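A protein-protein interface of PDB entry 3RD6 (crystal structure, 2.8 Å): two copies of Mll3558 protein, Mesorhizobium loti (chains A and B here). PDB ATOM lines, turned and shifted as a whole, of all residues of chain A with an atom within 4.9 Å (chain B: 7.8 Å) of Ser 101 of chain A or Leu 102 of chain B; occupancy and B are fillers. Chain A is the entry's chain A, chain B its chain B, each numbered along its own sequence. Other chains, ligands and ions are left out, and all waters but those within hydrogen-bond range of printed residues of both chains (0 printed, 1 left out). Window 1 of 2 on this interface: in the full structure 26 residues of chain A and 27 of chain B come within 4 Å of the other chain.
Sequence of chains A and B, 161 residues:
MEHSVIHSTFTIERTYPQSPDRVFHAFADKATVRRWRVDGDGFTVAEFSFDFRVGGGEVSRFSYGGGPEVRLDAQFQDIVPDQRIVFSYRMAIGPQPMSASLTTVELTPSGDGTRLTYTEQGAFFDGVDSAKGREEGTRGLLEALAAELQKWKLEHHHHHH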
ATOM      1  N   PHE A  87      22.138 -20.251 -23.546  1.00  0.00           N
ATOM      2  CA  PHE A  87      21.164 -19.964 -24.575  1.00  0.00           C
ATOM      3  C   PHE A  87      19.881 -20.736 -24.282  1.00  0.00           C
ATOM      4  O   PHE A  87      19.884 -21.764 -23.616  1.00  0.00           O
ATOM      5  CB  PHE A  87      21.693 -20.329 -25.978  1.00  0.00           C
ATOM      6  CG  PHE A  87      21.892 -21.815 -26.200  1.00  0.00           C
ATOM      7  CD1 PHE A  87      23.099 -22.418 -25.923  1.00  0.00           C
ATOM      8  CD2 PHE A  87      20.865 -22.601 -26.730  1.00  0.00           C
ATOM      9  CE1 PHE A  87      23.275 -23.767 -26.171  1.00  0.00           C
ATOM     10  CE2 PHE A  87      21.043 -23.960 -26.982  1.00  0.00           C
ATOM     11  CZ  PHE A  87      22.244 -24.536 -26.704  1.00  0.00           C
ATOM     12  N   SER A  88      18.781 -20.193 -24.765  1.00  0.00           N
ATOM     13  CA  SER A  88      17.473 -20.796 -24.634  1.00  0.00           C
ATOM     14  C   SER A  88      17.184 -21.255 -26.055  1.00  0.00           C
ATOM     15  O   SER A  88      17.859 -20.831 -26.997  1.00  0.00           O
ATOM     16  CB  SER A  88      16.441 -19.743 -24.232  1.00  0.00           C
ATOM     17  OG  SER A  88      16.340 -18.715 -25.206  1.00  0.00           O
ATOM     18  N   TYR A  89      16.194 -22.118 -26.215  1.00  0.00           N
ATOM     19  CA  TYR A  89      15.849 -22.584 -27.545  1.00  0.00           C
ATOM     20  C   TYR A  89      14.557 -23.338 -27.499  1.00  0.00           C
ATOM     21  O   TYR A  89      14.115 -23.752 -26.444  1.00  0.00           O
ATOM     22  CB  TYR A  89      16.962 -23.465 -28.138  1.00  0.00           C
ATOM     23  CG  TYR A  89      17.016 -24.883 -27.632  1.00  0.00           C
ATOM     24  CD1 TYR A  89      16.295 -25.891 -28.263  1.00  0.00           C
ATOM     25  CD2 TYR A  89      17.795 -25.222 -26.529  1.00  0.00           C
ATOM     26  CE1 TYR A  89      16.350 -27.203 -27.809  1.00  0.00           C
ATOM     27  CE2 TYR A  89      17.854 -26.531 -26.071  1.00  0.00           C
ATOM     28  CZ  TYR A  89      17.127 -27.516 -26.713  1.00  0.00           C
ATOM     29  OH  TYR A  89      17.153 -28.820 -26.280  1.00  0.00           O
ATOM     30  N   SER A  99       8.947 -28.557 -27.462  1.00  0.00           N
ATOM     31  CA  SER A  99       9.570 -28.064 -26.233  1.00  0.00           C
ATOM     32  C   SER A  99      10.341 -26.764 -26.337  1.00  0.00           C
ATOM     33  O   SER A  99      10.685 -26.324 -27.421  1.00  0.00           O
ATOM     34  CB  SER A  99      10.535 -29.107 -25.720  1.00  0.00           C
ATOM     35  OG  SER A  99      11.662 -29.158 -26.584  1.00  0.00           O
ATOM     36  N   ALA A 100      10.631 -26.186 -25.169  1.00  0.00           N
ATOM     37  CA  ALA A 100      11.419 -24.956 -25.023  1.00  0.00           C
ATOM     38  C   ALA A 100      12.299 -25.194 -23.814  1.00  0.00           C
ATOM     39  O   ALA A 100      11.856 -25.749 -22.823  1.00  0.00           O
ATOM     40  CB  ALA A 100      10.528 -23.756 -24.786  1.00  0.00           C
ATOM     41  N   SER A 101      13.553 -24.801 -23.893  1.00  0.00           N
ATOM     42  CA  SER A 101      14.438 -25.011 -22.771  1.00  0.00           C
ATOM     43  C   SER A 101      15.557 -23.993 -22.701  1.00  0.00           C
ATOM     44  O   SER A 101      15.699 -23.129 -23.556  1.00  0.00           O
ATOM     45  CB  SER A 101      15.005 -26.446 -22.788  1.00  0.00           C
ATOM     46  OG  SER A 101      15.070 -26.986 -24.078  1.00  0.00           O
ATOM     47  N   LEU A 102      16.330 -24.092 -21.639  1.00  0.00           N
ATOM     48  CA  LEU A 102      17.450 -23.215 -21.429  1.00  0.00           C
ATOM     49  C   LEU A 102      18.678 -24.110 -21.300  1.00  0.00           C
ATOM     50  O   LEU A 102      18.659 -25.122 -20.600  1.00  0.00           O
ATOM     51  CB  LEU A 102      17.248 -22.405 -20.149  1.00  0.00           C
ATOM     52  CG  LEU A 102      18.281 -21.309 -19.903  1.00  0.00           C
ATOM     53  CD1 LEU A 102      18.176 -20.281 -21.036  1.00  0.00           C
ATOM     54  CD2 LEU A 102      18.079 -20.653 -18.549  1.00  0.00           C
ATOM     55  N   THR A 103      19.735 -23.740 -22.008  1.00  0.00           N
ATOM     56  CA  THR A 103      20.974 -24.472 -21.964  1.00  0.00           C
ATOM     57  C   THR A 103      22.061 -23.623 -21.364  1.00  0.00           C
ATOM     58  O   THR A 103      22.132 -22.422 -21.585  1.00  0.00           O
ATOM     59  CB  THR A 103      21.427 -24.895 -23.338  1.00  0.00           C
ATOM     60  OG1 THR A 103      20.514 -25.872 -23.842  1.00  0.00           O
ATOM     61  CG2 THR A 103      22.818 -25.500 -23.280  1.00  0.00           C
ATOM     62  N   GLU A 120      20.752 -28.706 -18.935  1.00  0.00           N
ATOM     63  CA  GLU A 120      19.564 -28.328 -19.704  1.00  0.00           C
ATOM     64  C   GLU A 120      18.234 -28.330 -18.937  1.00  0.00           C
ATOM     65  O   GLU A 120      17.703 -29.386 -18.579  1.00  0.00           O
ATOM     66  CB  GLU A 120      19.440 -29.206 -20.960  1.00  0.00           C
ATOM     67  CG  GLU A 120      19.335 -28.361 -22.220  1.00  0.00           C
ATOM     68  CD  GLU A 120      19.376 -29.162 -23.504  1.00  0.00           C
ATOM     69  OE1 GLU A 120      18.371 -29.818 -23.823  1.00  0.00           O
ATOM     70  OE2 GLU A 120      20.419 -29.135 -24.196  1.00  0.00           O
ATOM     71  N   GLN A 121      17.706 -27.133 -18.685  1.00  0.00           N
ATOM     72  CA  GLN A 121      16.437 -26.988 -17.986  1.00  0.00           C
ATOM     73  C   GLN A 121      15.394 -26.871 -19.071  1.00  0.00           C
ATOM     74  O   GLN A 121      15.329 -25.867 -19.766  1.00  0.00           O
ATOM     75  CB  GLN A 121      16.460 -25.735 -17.113  1.00  0.00           C
ATOM     76  CG  GLN A 121      17.476 -25.806 -16.000  1.00  0.00           C
ATOM     77  CD  GLN A 121      17.802 -24.460 -15.407  1.00  0.00           C
ATOM     78  OE1 GLN A 121      18.491 -23.645 -16.022  1.00  0.00           O
ATOM     79  NE2 GLN A 121      17.308 -24.214 -14.203  1.00  0.00           N
ATOM     80  N   GLY A 122      14.591 -27.911 -19.229  1.00  0.00           N
ATOM     81  CA  GLY A 122      13.595 -27.876 -20.273  1.00  0.00           C
ATOM     82  C   GLY A 122      12.141 -27.964 -19.881  1.00  0.00           C
ATOM     83  O   GLY A 122      11.767 -28.348 -18.778  1.00  0.00           O
ATOM     84  N   ALA A 123      11.314 -27.582 -20.833  1.00  0.00           N
ATOM     85  CA  ALA A 123       9.875 -27.617 -20.691  1.00  0.00           C
ATOM     86  C   ALA A 123       9.369 -28.382 -21.919  1.00  0.00           C
ATOM     87  O   ALA A 123       9.427 -27.875 -23.042  1.00  0.00           O
ATOM     88  CB  ALA A 123       9.322 -26.184 -20.664  1.00  0.00           C
ATOM     89  N   ARG A 134      16.215 -36.542 -25.433  1.00  0.00           N
ATOM     90  CA  ARG A 134      17.046 -35.371 -25.655  1.00  0.00           C
ATOM     91  C   ARG A 134      18.365 -35.473 -24.899  1.00  0.00           C
ATOM     92  O   ARG A 134      19.405 -35.069 -25.426  1.00  0.00           O
ATOM     93  CB  ARG A 134      16.314 -34.087 -25.254  1.00  0.00           C
ATOM     94  CG  ARG A 134      16.906 -32.843 -25.905  1.00  0.00           C
ATOM     95  CD  ARG A 134      16.251 -31.552 -25.423  1.00  0.00           C
ATOM     96  NE  ARG A 134      14.817 -31.484 -25.696  1.00  0.00           N
ATOM     97  CZ  ARG A 134      14.271 -31.609 -26.899  1.00  0.00           C
ATOM     98  NH1 ARG A 134      15.037 -31.814 -27.953  1.00  0.00           N
ATOM     99  NH2 ARG A 134      12.958 -31.527 -27.047  1.00  0.00           N
ATOM    100  N   SER B   8      18.346 -23.517 -10.505  1.00  0.00           N
ATOM    101  CA  SER B   8      17.301 -23.865  -9.589  1.00  0.00           C
ATOM    102  C   SER B   8      16.005 -23.799 -10.355  1.00  0.00           C
ATOM    103  O   SER B   8      15.876 -23.074 -11.324  1.00  0.00           O
ATOM    104  CB  SER B   8      17.258 -22.882  -8.415  1.00  0.00           C
ATOM    105  OG  SER B   8      16.656 -21.649  -8.777  1.00  0.00           O
ATOM    106  N   THR B   9      15.045 -24.589  -9.929  1.00  0.00           N
ATOM    107  CA  THR B   9      13.750 -24.570 -10.562  1.00  0.00           C
ATOM    108  C   THR B   9      12.839 -24.464  -9.369  1.00  0.00           C
ATOM    109  O   THR B   9      12.979 -25.219  -8.406  1.00  0.00           O
ATOM    110  CB  THR B   9      13.426 -25.892 -11.302  1.00  0.00           C
ATOM    111  OG1 THR B   9      14.447 -26.187 -12.269  1.00  0.00           O
ATOM    112  CG2 THR B   9      12.078 -25.783 -12.007  1.00  0.00           C
ATOM    113  N   PHE B  10      11.945 -23.494  -9.394  1.00  0.00           N
ATOM    114  CA  PHE B  10      11.007 -23.357  -8.307  1.00  0.00           C
ATOM    115  C   PHE B  10       9.657 -23.162  -8.959  1.00  0.00           C
ATOM    116  O   PHE B  10       9.520 -22.436  -9.948  1.00  0.00           O
ATOM    117  CB  PHE B  10      11.364 -22.174  -7.379  1.00  0.00           C
ATOM    118  CG  PHE B  10      11.203 -20.816  -8.011  1.00  0.00           C
ATOM    119  CD1 PHE B  10       9.939 -20.306  -8.309  1.00  0.00           C
ATOM    120  CD2 PHE B  10      12.322 -20.053  -8.335  1.00  0.00           C
ATOM    121  CE1 PHE B  10       9.789 -19.065  -8.925  1.00  0.00           C
ATOM    122  CE2 PHE B  10      12.181 -18.808  -8.950  1.00  0.00           C
ATOM    123  CZ  PHE B  10      10.911 -18.318  -9.244  1.00  0.00           C
ATOM    124  N   GLN B  75      12.022 -13.479 -24.615  1.00  0.00           N
ATOM    125  CA  GLN B  75      11.569 -13.937 -25.916  1.00  0.00           C
ATOM    126  C   GLN B  75      10.541 -15.053 -25.701  1.00  0.00           C
ATOM    127  O   GLN B  75      10.808 -16.044 -25.020  1.00  0.00           O
ATOM    128  CB  GLN B  75      12.748 -14.437 -26.757  1.00  0.00           C
ATOM    129  CG  GLN B  75      12.384 -14.544 -28.228  1.00  0.00           C
ATOM    130  CD  GLN B  75      13.433 -15.214 -29.078  1.00  0.00           C
ATOM    131  OE1 GLN B  75      14.556 -14.734 -29.202  1.00  0.00           O
ATOM    132  NE2 GLN B  75      13.066 -16.336 -29.674  1.00  0.00           N
ATOM    133  N   PHE B  76       9.350 -14.875 -26.259  1.00  0.00           N
ATOM    134  CA  PHE B  76       8.292 -15.870 -26.112  1.00  0.00           C
ATOM    135  C   PHE B  76       8.596 -17.144 -26.909  1.00  0.00           C
ATOM    136  O   PHE B  76       8.799 -17.099 -28.127  1.00  0.00           O
ATOM    137  CB  PHE B  76       6.944 -15.279 -26.526  1.00  0.00           C
ATOM    138  CG  PHE B  76       6.451 -14.200 -25.603  1.00  0.00           C
ATOM    139  CD1 PHE B  76       6.072 -14.502 -24.302  1.00  0.00           C
ATOM    140  CD2 PHE B  76       6.380 -12.878 -26.027  1.00  0.00           C
ATOM    141  CE1 PHE B  76       5.631 -13.507 -23.434  1.00  0.00           C
ATOM    142  CE2 PHE B  76       5.939 -11.875 -25.160  1.00  0.00           C
ATOM    143  CZ  PHE B  76       5.566 -12.192 -23.863  1.00  0.00           C
ATOM    144  N   GLN B  77       8.650 -18.263 -26.184  1.00  0.00           N
ATOM    145  CA  GLN B  77       8.937 -19.572 -26.751  1.00  0.00           C
ATOM    146  C   GLN B  77       7.681 -20.328 -27.196  1.00  0.00           C
ATOM    147  O   GLN B  77       7.628 -20.842 -28.305  1.00  0.00           O
ATOM    148  CB  GLN B  77       9.706 -20.411 -25.727  1.00  0.00           C
ATOM    149  CG  GLN B  77      11.031 -19.830 -25.283  1.00  0.00           C
ATOM    150  CD  GLN B  77      11.941 -19.462 -26.458  1.00  0.00           C
ATOM    151  OE1 GLN B  77      12.033 -20.191 -27.445  1.00  0.00           O
ATOM    152  NE2 GLN B  77      12.628 -18.330 -26.345  1.00  0.00           N
ATOM    153  N   ASP B  78       6.679 -20.381 -26.318  1.00  0.00           N
ATOM    154  CA  ASP B  78       5.437 -21.093 -26.592  1.00  0.00           C
ATOM    155  C   ASP B  78       4.208 -20.362 -26.042  1.00  0.00           C
ATOM    156  O   ASP B  78       4.185 -19.989 -24.869  1.00  0.00           O
ATOM    157  CB  ASP B  78       5.479 -22.504 -25.977  1.00  0.00           C
ATOM    158  CG  ASP B  78       4.354 -23.394 -26.483  1.00  0.00           C
ATOM    159  OD1 ASP B  78       4.546 -23.989 -27.563  1.00  0.00           O
ATOM    160  OD2 ASP B  78       3.292 -23.506 -25.812  1.00  0.00           O
ATOM    161  N   ILE B  85       1.835 -19.767 -21.279  1.00  0.00           N
ATOM    162  CA  ILE B  85       2.784 -18.748 -21.722  1.00  0.00           C
ATOM    163  C   ILE B  85       4.190 -19.179 -21.326  1.00  0.00           C
ATOM    164  O   ILE B  85       4.488 -19.343 -20.146  1.00  0.00           O
ATOM    165  CB  ILE B  85       2.508 -17.399 -21.077  1.00  0.00           C
ATOM    166  CG1 ILE B  85       1.059 -16.997 -21.349  1.00  0.00           C
ATOM    167  CG2 ILE B  85       3.508 -16.367 -21.586  1.00  0.00           C
ATOM    168  CD1 ILE B  85       0.599 -15.849 -20.533  1.00  0.00           C
ATOM    169  N   VAL B  86       5.034 -19.410 -22.320  1.00  0.00           N
ATOM    170  CA  VAL B  86       6.407 -19.830 -22.065  1.00  0.00           C
ATOM    171  C   VAL B  86       7.324 -18.794 -22.678  1.00  0.00           C
ATOM    172  O   VAL B  86       7.196 -18.450 -23.854  1.00  0.00           O
ATOM    173  CB  VAL B  86       6.747 -21.202 -22.716  1.00  0.00           C
ATOM    174  CG1 VAL B  86       8.079 -21.693 -22.209  1.00  0.00           C
ATOM    175  CG2 VAL B  86       5.660 -22.211 -22.461  1.00  0.00           C
ATOM    176  N   PHE B  87       8.235 -18.273 -21.872  1.00  0.00           N
ATOM    177  CA  PHE B  87       9.182 -17.292 -22.374  1.00  0.00           C
ATOM    178  C   PHE B  87      10.506 -17.403 -21.648  1.00  0.00           C
ATOM    179  O   PHE B  87      10.586 -17.894 -20.515  1.00  0.00           O
ATOM    180  CB  PHE B  87       8.634 -15.862 -22.241  1.00  0.00           C
ATOM    181  CG  PHE B  87       8.488 -15.378 -20.815  1.00  0.00           C
ATOM    182  CD1 PHE B  87       7.286 -15.553 -20.119  1.00  0.00           C
ATOM    183  CD2 PHE B  87       9.539 -14.727 -20.173  1.00  0.00           C
ATOM    184  CE1 PHE B  87       7.130 -15.086 -18.809  1.00  0.00           C
ATOM    185  CE2 PHE B  87       9.383 -14.261 -18.859  1.00  0.00           C
ATOM    186  CZ  PHE B  87       8.187 -14.437 -18.180  1.00  0.00           C
ATOM    187  N   SER B  88      11.558 -16.986 -22.336  1.00  0.00           N
ATOM    188  CA  SER B  88      12.879 -17.004 -21.746  1.00  0.00           C
ATOM    189  C   SER B  88      13.135 -15.525 -21.511  1.00  0.00           C
ATOM    190  O   SER B  88      12.424 -14.664 -22.055  1.00  0.00           O
ATOM    191  CB  SER B  88      13.911 -17.564 -22.714  1.00  0.00           C
ATOM    192  OG  SER B  88      13.997 -16.759 -23.865  1.00  0.00           O
ATOM    193  N   TYR B  89      14.116 -15.225 -20.671  1.00  0.00           N
ATOM    194  CA  TYR B  89      14.457 -13.849 -20.406  1.00  0.00           C
ATOM    195  C   TYR B  89      15.755 -13.742 -19.623  1.00  0.00           C
ATOM    196  O   TYR B  89      16.180 -14.677 -18.943  1.00  0.00           O
ATOM    197  CB  TYR B  89      13.307 -13.136 -19.675  1.00  0.00           C
ATOM    198  CG  TYR B  89      13.253 -13.347 -18.191  1.00  0.00           C
ATOM    199  CD1 TYR B  89      13.996 -12.544 -17.334  1.00  0.00           C
ATOM    200  CD2 TYR B  89      12.455 -14.342 -17.637  1.00  0.00           C
ATOM    201  CE1 TYR B  89      13.936 -12.716 -15.949  1.00  0.00           C
ATOM    202  CE2 TYR B  89      12.400 -14.534 -16.267  1.00  0.00           C
ATOM    203  CZ  TYR B  89      13.137 -13.719 -15.420  1.00  0.00           C
ATOM    204  OH  TYR B  89      13.056 -13.907 -14.057  1.00  0.00           O
ATOM    205  N   ARG B  90      16.391 -12.589 -19.750  1.00  0.00           N
ATOM    206  CA  ARG B  90      17.623 -12.334 -19.068  1.00  0.00           C
ATOM    207  C   ARG B  90      17.509 -10.965 -18.439  1.00  0.00           C
ATOM    208  O   ARG B  90      16.829 -10.091 -18.942  1.00  0.00           O
ATOM    209  CB  ARG B  90      18.806 -12.422 -20.046  1.00  0.00           C
ATOM    210  CG  ARG B  90      18.673 -11.589 -21.278  1.00  0.00           C
ATOM    211  CD  ARG B  90      19.940 -11.660 -22.097  1.00  0.00           C
ATOM    212  NE  ARG B  90      19.972 -10.689 -23.197  1.00  0.00           N
ATOM    213  CZ  ARG B  90      19.360 -10.853 -24.361  1.00  0.00           C
ATOM    214  NH1 ARG B  90      18.659 -11.944 -24.610  1.00  0.00           N
ATOM    215  NH2 ARG B  90      19.462  -9.920 -25.275  1.00  0.00           N
ATOM    216  N   ALA B 100      19.482 -15.637 -16.519  1.00  0.00           N
ATOM    217  CA  ALA B 100      18.698 -15.980 -17.711  1.00  0.00           C
ATOM    218  C   ALA B 100      17.802 -17.135 -17.292  1.00  0.00           C
ATOM    219  O   ALA B 100      18.264 -18.056 -16.593  1.00  0.00           O
ATOM    220  CB  ALA B 100      19.596 -16.431 -18.835  1.00  0.00           C
ATOM    221  N   SER B 101      16.529 -17.096 -17.678  1.00  0.00           N
ATOM    222  CA  SER B 101      15.658 -18.191 -17.289  1.00  0.00           C
ATOM    223  C   SER B 101      14.532 -18.480 -18.253  1.00  0.00           C
ATOM    224  O   SER B 101      14.194 -17.665 -19.097  1.00  0.00           O
ATOM    225  CB  SER B 101      15.094 -17.930 -15.889  1.00  0.00           C
ATOM    226  OG  SER B 101      14.374 -16.718 -15.866  1.00  0.00           O
ATOM    227  N   LEU B 102      13.977 -19.679 -18.128  1.00  0.00           N
ATOM    228  CA  LEU B 102      12.854 -20.102 -18.951  1.00  0.00           C
ATOM    229  C   LEU B 102      11.648 -20.102 -18.033  1.00  0.00           C
ATOM    230  O   LEU B 102      11.647 -20.787 -17.002  1.00  0.00           O
ATOM    231  CB  LEU B 102      13.068 -21.506 -19.510  1.00  0.00           C
ATOM    232  CG  LEU B 102      11.876 -21.945 -20.347  1.00  0.00           C
ATOM    233  CD1 LEU B 102      11.734 -21.040 -21.532  1.00  0.00           C
ATOM    234  CD2 LEU B 102      12.040 -23.375 -20.779  1.00  0.00           C
ATOM    235  N   THR B 103      10.635 -19.317 -18.380  1.00  0.00           N
ATOM    236  CA  THR B 103       9.468 -19.228 -17.526  1.00  0.00           C
ATOM    237  C   THR B 103       8.211 -19.834 -18.104  1.00  0.00           C
ATOM    238  O   THR B 103       7.837 -19.567 -19.250  1.00  0.00           O
ATOM    239  CB  THR B 103       9.187 -17.764 -17.125  1.00  0.00           C
ATOM    240  OG1 THR B 103      10.197 -17.334 -16.196  1.00  0.00           O
ATOM    241  CG2 THR B 103       7.790 -17.621 -16.494  1.00  0.00           C
ATOM    242  N   THR B 104       7.570 -20.669 -17.292  1.00  0.00           N
ATOM    243  CA  THR B 104       6.328 -21.302 -17.695  1.00  0.00           C
ATOM    244  C   THR B 104       5.251 -20.799 -16.755  1.00  0.00           C
ATOM    245  O   THR B 104       5.424 -20.812 -15.528  1.00  0.00           O
ATOM    246  CB  THR B 104       6.370 -22.846 -17.575  1.00  0.00           C
ATOM    247  OG1 THR B 104       7.583 -23.353 -18.137  1.00  0.00           O
ATOM    248  CG2 THR B 104       5.186 -23.440 -18.299  1.00  0.00           C
ATOM    249  N   VAL B 105       4.163 -20.320 -17.337  1.00  0.00           N
ATOM    250  CA  VAL B 105       3.033 -19.854 -16.557  1.00  0.00           C
ATOM    251  C   VAL B 105       1.828 -20.590 -17.134  1.00  0.00           C
ATOM    252  O   VAL B 105       1.421 -20.364 -18.285  1.00  0.00           O
ATOM    253  CB  VAL B 105       2.847 -18.295 -16.626  1.00  0.00           C
ATOM    254  CG1 VAL B 105       2.930 -17.811 -18.048  1.00  0.00           C
ATOM    255  CG2 VAL B 105       1.499 -17.894 -16.025  1.00  0.00           C
ATOM    256  N   THR B 119       6.131 -21.391 -13.090  1.00  0.00           N
ATOM    257  CA  THR B 119       7.349 -22.165 -13.057  1.00  0.00           C
ATOM    258  C   THR B 119       8.485 -21.368 -13.660  1.00  0.00           C
ATOM    259  O   THR B 119       8.341 -20.752 -14.726  1.00  0.00           O
ATOM    260  CB  THR B 119       7.234 -23.487 -13.845  1.00  0.00           C
ATOM    261  OG1 THR B 119       6.080 -24.229 -13.417  1.00  0.00           O
ATOM    262  CG2 THR B 119       8.512 -24.319 -13.612  1.00  0.00           C
ATOM    263  N   GLU B 120       9.614 -21.386 -12.969  1.00  0.00           N
ATOM    264  CA  GLU B 120      10.772 -20.681 -13.445  1.00  0.00           C
ATOM    265  C   GLU B 120      12.004 -21.543 -13.285  1.00  0.00           C
ATOM    266  O   GLU B 120      12.375 -21.947 -12.171  1.00  0.00           O
ATOM    267  CB  GLU B 120      10.951 -19.384 -12.678  1.00  0.00           C
ATOM    268  CG  GLU B 120      11.780 -18.370 -13.434  1.00  0.00           C
ATOM    269  CD  GLU B 120      11.985 -17.101 -12.660  1.00  0.00           C
ATOM    270  OE1 GLU B 120      12.809 -17.116 -11.720  1.00  0.00           O
ATOM    271  OE2 GLU B 120      11.309 -16.101 -12.987  1.00  0.00           O
ATOM    272  N   GLN B 121      12.612 -21.847 -14.425  1.00  0.00           N
ATOM    273  CA  GLN B 121      13.826 -22.637 -14.469  1.00  0.00           C
ATOM    274  C   GLN B 121      14.865 -21.567 -14.762  1.00  0.00           C
ATOM    275  O   GLN B 121      14.855 -20.959 -15.832  1.00  0.00           O
ATOM    276  CB  GLN B 121      13.712 -23.677 -15.580  1.00  0.00           C
ATOM    277  CG  GLN B 121      12.467 -24.563 -15.431  1.00  0.00           C
ATOM    278  CD  GLN B 121      12.144 -25.370 -16.669  1.00  0.00           C
ATOM    279  OE1 GLN B 121      11.484 -24.873 -17.576  1.00  0.00           O
ATOM    280  NE2 GLN B 121      12.617 -26.622 -16.714  1.00  0.00           N
ATOM    281  N   GLY B 122      15.730 -21.311 -13.784  1.00  0.00           N
ATOM    282  CA  GLY B 122      16.705 -20.264 -13.949  1.00  0.00           C
ATOM    283  C   GLY B 122      18.156 -20.624 -13.780  1.00  0.00           C
ATOM    284  O   GLY B 122      18.501 -21.691 -13.298  1.00  0.00           O
ATOM    285  N   ALA B 123      19.001 -19.697 -14.213  1.00  0.00           N
ATOM    286  CA  ALA B 123      20.450 -19.810 -14.139  1.00  0.00           C
ATOM    287  C   ALA B 123      20.916 -18.496 -13.511  1.00  0.00           C
ATOM    288  O   ALA B 123      20.655 -17.424 -14.049  1.00  0.00           O
ATOM    289  CB  ALA B 123      21.032 -19.963 -15.535  1.00  0.00           C
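The side-chain hydroxyl (OG) of Ser 88 of chain B is in hydrogen-bond range of the side-chain hydroxyl (OG) of Ser 88 of chain A, 3.3 Å away.
The backbone carbonyl oxygen (O) of Ser 8 of chain B lies within hydrogen-bond range of the side-chain amide nitrogen (NE2) of Gln 121 of chain A.
The backbone carbonyl oxygen (O) of Gly 122 of chain B is in hydrogen-bond range of the side-chain amide nitrogen (NE2) of Gln 121 of chain A, 2.9 Å away.
O of Gly 122 of chain A lies within hydrogen-bond range of NE2 of Gln 121 of chain B, at 2.8 Å.
The backbone NH (N) of Ala 123 of chain A lies within hydrogen-bond range of the backbone carbonyl oxygen (O) of Ala 100 of chain A (2.8 Å).
O of Ser 8 of chain B lies within hydrogen-bond range of N of Gly 122 of chain B, at 3.0 Å.
The side-chain amide nitrogen (NE2) of Gln 77 of chain B sits at hydrogen-bond distance from the backbone carbonyl oxygen (O) of Gln 75 of chain B, 3.2 Å away.
The backbone NH (N) of Gln 75 of chain B is in hydrogen-bond range of the backbone carbonyl oxygen (O) of Ser 88 of chain B.
OG of Ser 88 of chain B sits at hydrogen-bond distance from NE2 of Gln 77 of chain B (3.2 Å).
The backbone NH (N) of Ser 101 of chain B sits at hydrogen-bond distance from the backbone carbonyl oxygen (O) of Tyr 89 of chain B.
Among the printed residues, merely in contact across the chains: Ala 100 of chain A with Leu 102 of chain B (3.1 Å), Leu 102 of chain A with Ala 100 of chain B (3.3 Å), Ser 101 of chain A with Leu 102 of chain B (3.5 Å), Ala 100 of chain A with Gln 77 of chain B (3.6 Å), Gln 121 of chain A with Gln 121 of chain B (3.6 Å), Leu 102 of chain A with Ser 101 of chain B (3.7 Å), Ser 88 of chain A with Gln 77 of chain B (3.9 Å), Ala 123 of chain A with Leu 102 of chain B (3.9 Å), Gln 121 of chain A with Thr 9 of chain B (3.98 Å) and Ala 123 of chain A with Gln 121 of chain B (3.99 Å).
Ser 101 of chain A touches one residue of chain B.
Leu 102 of chain B touches three residues of chain A.
Ala 100 of chain A touches just these residues of chain B: Gln 77 (3.6 Å) and Leu 102 (3.1 Å).
Printed residues of chain A within 4 Å of Thr 9 of chain B: Gln 121 (3.98 Å).
Printed residues of chain B within 4 Å of Gly 122 of chain A: Gln 121.
Thr 103 of chain B touches none of the printed residues of chain A.
Ala 123 of chain B touches none of the printed residues of chain A.
The nearest residue of chain B that does not touch Ser 101 of chain A is Gln 77 of chain B (5.7 Å).
Of the 13 printed residues of chain A, 7 touch a printed residue of chain B.
Printed residues of chain B that touch a printed residue of chain A: Ser 8, Thr 9, Gln 77, Ser 88, Ala 100, Ser 101, Leu 102, Gln 121 and Gly 122.
Hydrophobic or aromatic side chains of chain B within 4 Å of the printed part of chain A: Leu 102.
Among the printed residues, 14 pairs touch across the chains.
Ala 100 of chain A touches Leu 102 of chain B, and with the chains exchanged Leu 102 of chain A touches Ala 100 of chain B.
Ser 101 of chain A touches Leu 102 of chain B, and with the chains exchanged Leu 102 of chain A touches Ser 101 of chain B.
Ala 123 of chain A touches Leu 102 of chain B, but with the chains exchanged Leu 102 of chain A does not touch Ala 123 of chain B (4.3 Å).
Ala 123 of chain A touches Gln 121 of chain B, but with the chains exchanged Gln 121 of chain A does not touch Ala 123 of chain B (4.4 Å).
Of the 14 pairs that touch across the chains among the printed residues, 8 have their exchanged pair printed and touching as well.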
